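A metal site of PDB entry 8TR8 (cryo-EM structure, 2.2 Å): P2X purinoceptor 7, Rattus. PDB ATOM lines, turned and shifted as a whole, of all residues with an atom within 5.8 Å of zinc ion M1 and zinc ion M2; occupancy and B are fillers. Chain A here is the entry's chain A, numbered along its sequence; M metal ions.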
ATOM      1  N   TRP A 476       1.946 -32.690  -9.211  1.00  0.00           N
ATOM      2  CA  TRP A 476       2.020 -31.382  -8.549  1.00  0.00           C
ATOM      3  C   TRP A 476       1.806 -30.239  -9.531  1.00  0.00           C
ATOM      4  O   TRP A 476       1.374 -29.159  -9.134  1.00  0.00           O
ATOM      5  CB  TRP A 476       3.363 -31.230  -7.838  1.00  0.00           C
ATOM      6  CG  TRP A 476       4.539 -31.692  -8.613  1.00  0.00           C
ATOM      7  CD1 TRP A 476       5.173 -32.891  -8.501  1.00  0.00           C
ATOM      8  CD2 TRP A 476       5.241 -30.980  -9.636  1.00  0.00           C
ATOM      9  NE1 TRP A 476       6.226 -32.963  -9.375  1.00  0.00           N
ATOM     10  CE2 TRP A 476       6.290 -31.804 -10.091  1.00  0.00           C
ATOM     11  CE3 TRP A 476       5.084 -29.717 -10.219  1.00  0.00           C
ATOM     12  CZ2 TRP A 476       7.162 -31.410 -11.088  1.00  0.00           C
ATOM     13  CZ3 TRP A 476       5.959 -29.322 -11.206  1.00  0.00           C
ATOM     14  CH2 TRP A 476       6.980 -30.172 -11.630  1.00  0.00           C
ATOM     15  N   CYS A 477       2.101 -30.462 -10.808  1.00  0.00           N
ATOM     16  CA  CYS A 477       1.896 -29.420 -11.803  1.00  0.00           C
ATOM     17  C   CYS A 477       0.413 -29.116 -11.969  1.00  0.00           C
ATOM     18  O   CYS A 477      -0.428 -30.017 -11.962  1.00  0.00           O
ATOM     19  CB  CYS A 477       2.494 -29.838 -13.154  1.00  0.00           C
ATOM     20  SG  CYS A 477       2.121 -28.704 -14.498  1.00  0.00           S
ATOM     21  N   GLN A 478       0.108 -27.826 -12.128  1.00  0.00           N
ATOM     22  CA  GLN A 478      -1.247 -27.358 -12.377  1.00  0.00           C
ATOM     23  C   GLN A 478      -1.294 -26.438 -13.591  1.00  0.00           C
ATOM     24  O   GLN A 478      -2.164 -25.576 -13.689  1.00  0.00           O
ATOM     25  CB  GLN A 478      -1.825 -26.650 -11.154  1.00  0.00           C
ATOM     26  CG  GLN A 478      -1.218 -27.014  -9.805  1.00  0.00           C
ATOM     27  CD  GLN A 478      -1.859 -28.248  -9.184  1.00  0.00           C
ATOM     28  OE1 GLN A 478      -2.930 -28.684  -9.608  1.00  0.00           O
ATOM     29  NE2 GLN A 478      -1.200 -28.805  -8.174  1.00  0.00           N
ATOM     30  N   CYS A 479      -0.351 -26.612 -14.519  1.00  0.00           N
ATOM     31  CA  CYS A 479      -0.296 -25.779 -15.711  1.00  0.00           C
ATOM     32  C   CYS A 479      -0.142 -26.554 -17.009  1.00  0.00           C
ATOM     33  O   CYS A 479      -0.374 -25.974 -18.076  1.00  0.00           O
ATOM     34  CB  CYS A 479       0.866 -24.772 -15.597  1.00  0.00           C
ATOM     35  SG  CYS A 479       2.496 -25.370 -16.109  1.00  0.00           S
ATOM     36  N   GLY A 480       0.224 -27.832 -16.961  1.00  0.00           N
ATOM     37  CA  GLY A 480       0.297 -28.655 -18.139  1.00  0.00           C
ATOM     38  C   GLY A 480       1.572 -28.505 -18.950  1.00  0.00           C
ATOM     39  O   GLY A 480       1.707 -29.183 -19.982  1.00  0.00           O
ATOM     40  N   ASN A 481       2.498 -27.651 -18.528  1.00  0.00           N
ATOM     41  CA  ASN A 481       3.735 -27.426 -19.264  1.00  0.00           C
ATOM     42  C   ASN A 481       4.976 -27.854 -18.498  1.00  0.00           C
ATOM     43  O   ASN A 481       6.061 -27.900 -19.103  1.00  0.00           O
ATOM     44  CB  ASN A 481       3.868 -25.939 -19.625  1.00  0.00           C
ATOM     45  CG  ASN A 481       2.587 -25.359 -20.186  1.00  0.00           C
ATOM     46  OD1 ASN A 481       1.653 -25.065 -19.450  1.00  0.00           O
ATOM     47  ND2 ASN A 481       2.550 -25.193 -21.505  1.00  0.00           N
ATOM     48  N   CYS A 482       4.860 -28.184 -17.215  1.00  0.00           N
ATOM     49  CA  CYS A 482       6.016 -28.613 -16.447  1.00  0.00           C
ATOM     50  C   CYS A 482       6.448 -30.013 -16.853  1.00  0.00           C
ATOM     51  O   CYS A 482       5.660 -30.815 -17.381  1.00  0.00           O
ATOM     52  CB  CYS A 482       5.691 -28.577 -14.956  1.00  0.00           C
ATOM     53  SG  CYS A 482       5.461 -26.922 -14.276  1.00  0.00           S
ATOM     54  N   LEU A 497       8.481 -27.880  -9.008  1.00  0.00           N
ATOM     55  CA  LEU A 497       7.757 -26.649  -8.714  1.00  0.00           C
ATOM     56  C   LEU A 497       7.002 -26.196  -9.948  1.00  0.00           C
ATOM     57  O   LEU A 497       7.516 -26.287 -11.069  1.00  0.00           O
ATOM     58  CB  LEU A 497       8.719 -25.569  -8.241  1.00  0.00           C
ATOM     59  CG  LEU A 497       8.174 -24.197  -7.843  1.00  0.00           C
ATOM     60  CD1 LEU A 497       7.362 -24.279  -6.571  1.00  0.00           C
ATOM     61  CD2 LEU A 497       9.323 -23.235  -7.701  1.00  0.00           C
ATOM     62  N   CYS A 498       5.781 -25.711  -9.735  1.00  0.00           N
ATOM     63  CA  CYS A 498       4.936 -25.213 -10.803  1.00  0.00           C
ATOM     64  C   CYS A 498       4.696 -23.721 -10.615  1.00  0.00           C
ATOM     65  O   CYS A 498       4.856 -23.173  -9.526  1.00  0.00           O
ATOM     66  CB  CYS A 498       3.591 -25.965 -10.860  1.00  0.00           C
ATOM     67  SG  CYS A 498       2.545 -25.559 -12.281  1.00  0.00           S
ATOM     68  N   CYS A 499       4.316 -23.066 -11.722  1.00  0.00           N
ATOM     69  CA  CYS A 499       4.022 -21.644 -11.700  1.00  0.00           C
ATOM     70  C   CYS A 499       2.823 -21.288 -10.834  1.00  0.00           C
ATOM     71  O   CYS A 499       2.652 -20.104 -10.520  1.00  0.00           O
ATOM     72  CB  CYS A 499       3.778 -21.151 -13.129  1.00  0.00           C
ATOM     73  SG  CYS A 499       2.611 -22.143 -14.076  1.00  0.00           S
ATOM     74  N   ARG A 500       1.991 -22.259 -10.458  1.00  0.00           N
ATOM     75  CA  ARG A 500       0.760 -21.957  -9.745  1.00  0.00           C
ATOM     76  C   ARG A 500       0.417 -23.118  -8.817  1.00  0.00           C
ATOM     77  O   ARG A 500       0.893 -24.242  -8.992  1.00  0.00           O
ATOM     78  CB  ARG A 500      -0.382 -21.696 -10.708  1.00  0.00           C
ATOM     79  CG  ARG A 500      -0.570 -22.775 -11.747  1.00  0.00           C
ATOM     80  CD  ARG A 500      -1.514 -22.344 -12.844  1.00  0.00           C
ATOM     81  NE  ARG A 500      -2.518 -21.405 -12.361  1.00  0.00           N
ATOM     82  CZ  ARG A 500      -2.931 -20.333 -13.021  1.00  0.00           C
ATOM     83  NH1 ARG A 500      -2.424 -20.025 -14.200  1.00  0.00           N
ATOM     84  NH2 ARG A 500      -3.850 -19.546 -12.483  1.00  0.00           N
ATOM     85  N   CYS A 506      -0.641 -21.352 -17.848  1.00  0.00           N
ATOM     86  CA  CYS A 506       0.751 -21.176 -17.454  1.00  0.00           C
ATOM     87  C   CYS A 506       1.189 -19.732 -17.655  1.00  0.00           C
ATOM     88  O   CYS A 506       0.727 -19.030 -18.567  1.00  0.00           O
ATOM     89  CB  CYS A 506       1.652 -22.120 -18.253  1.00  0.00           C
ATOM     90  SG  CYS A 506       3.389 -22.072 -17.774  1.00  0.00           S
ATOM     91  N   ILE A 507       2.107 -19.280 -16.795  1.00  0.00           N
ATOM     92  CA  ILE A 507       2.649 -17.930 -16.900  1.00  0.00           C
ATOM     93  C   ILE A 507       3.379 -17.747 -18.222  1.00  0.00           C
ATOM     94  O   ILE A 507       3.479 -16.623 -18.736  1.00  0.00           O
ATOM     95  CB  ILE A 507       3.568 -17.642 -15.702  1.00  0.00           C
ATOM     96  CG1 ILE A 507       4.029 -16.176 -15.734  1.00  0.00           C
ATOM     97  CG2 ILE A 507       4.765 -18.570 -15.708  1.00  0.00           C
ATOM     98  CD1 ILE A 507       4.601 -15.694 -14.428  1.00  0.00           C
ATOM     99  N   THR A 508       3.907 -18.828 -18.801  1.00  0.00           N
ATOM    100  CA  THR A 508       4.620 -18.730 -20.068  1.00  0.00           C
ATOM    101  C   THR A 508       3.752 -18.209 -21.195  1.00  0.00           C
ATOM    102  O   THR A 508       4.274 -17.685 -22.181  1.00  0.00           O
ATOM    103  CB  THR A 508       5.186 -20.096 -20.462  1.00  0.00           C
ATOM    104  OG1 THR A 508       4.114 -21.048 -20.553  1.00  0.00           O
ATOM    105  CG2 THR A 508       6.188 -20.576 -19.428  1.00  0.00           C
ATOM    106  N   PRO A 570       9.983 -22.057 -11.654  1.00  0.00           N
ATOM    107  CA  PRO A 570       9.111 -23.193 -11.979  1.00  0.00           C
ATOM    108  C   PRO A 570       9.688 -24.032 -13.095  1.00  0.00           C
ATOM    109  O   PRO A 570      10.477 -23.581 -13.929  1.00  0.00           O
ATOM    110  CB  PRO A 570       7.797 -22.524 -12.395  1.00  0.00           C
ATOM    111  CG  PRO A 570       7.872 -21.158 -11.864  1.00  0.00           C
ATOM    112  CD  PRO A 570       9.301 -20.780 -11.865  1.00  0.00           C
ATOM    113  N   CYS A 572       8.192 -25.333 -15.723  1.00  0.00           N
ATOM    114  CA  CYS A 572       7.760 -24.915 -17.052  1.00  0.00           C
ATOM    115  C   CYS A 572       8.645 -23.813 -17.612  1.00  0.00           C
ATOM    116  O   CYS A 572       9.160 -23.915 -18.732  1.00  0.00           O
ATOM    117  CB  CYS A 572       6.299 -24.465 -16.989  1.00  0.00           C
ATOM    118  SG  CYS A 572       5.870 -23.607 -15.468  1.00  0.00           S
ATOM    119  N   CYS A 573       8.818 -22.736 -16.840  1.00  0.00           N
ATOM    120  CA  CYS A 573       9.644 -21.614 -17.292  1.00  0.00           C
ATOM    121  C   CYS A 573      11.084 -22.053 -17.486  1.00  0.00           C
ATOM    122  O   CYS A 573      11.743 -21.681 -18.463  1.00  0.00           O
ATOM    123  CB  CYS A 573       9.546 -20.483 -16.273  1.00  0.00           C
ATOM    124  SG  CYS A 573       7.865 -20.205 -15.685  1.00  0.00           S
HETATM  125 ZN    ZN M   1       3.156 -26.622 -14.259  1.00  0.00          ZN
HETATM  126 ZN    ZN M   2       3.585 -23.325 -15.829  1.00  0.00          ZN
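The side-chain hydroxyl of Thr 508 lies close to the side-chain sulfur of Cys 506, at 3.0 Å. SG of Cys 482 lies close to N of Cys 572, 3.5 Å away. The side-chain sulfur (SG) of Cys 498 sits close to the backbone NH (N) of Gln 478. The backbone carbonyl oxygen (O) of Cys 479 lies close to the side-chain amide oxygen (OD1) of Asn 481. The side-chain sulfur (SG) of Cys 477 sits close to the backbone NH (N) of Gly 480. The backbone carbonyl oxygen (O) of Trp 476 lies within hydrogen-bond range of the side-chain amide nitrogen (NE2) of Gln 478, 2.8 Å away.
Zinc ion M1 is bound by the side-chain sulfur (SG) of Cys 482, the side-chain sulfur (SG) of Cys 498, the side-chain sulfur (SG) of Cys 479 and the side-chain sulfur (SG) of Cys 477. Zinc ion M1 has four donor atoms within binding distance.
Gln 478 touches zinc ion M1 (N to ZN, 3.9 Å). Within 4 Å of zinc ion M1: Cys 477, Gln 478, Cys 479, Cys 482 and Cys 498. The nearest printed residue that does not touch zinc ion M1 is Gly 480 (4.2 Å).
Zinc ion M2 is bound by SG of Cys 506 (2.3 Å). The side-chain sulfur (SG) of Cys 499 binds zinc ion M2, 2.3 Å away. The side-chain sulfur (SG) of Cys 572 binds zinc ion M2 (2.3 Å). Zinc ion M2 is bound by SG of Cys 479 (2.3 Å).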
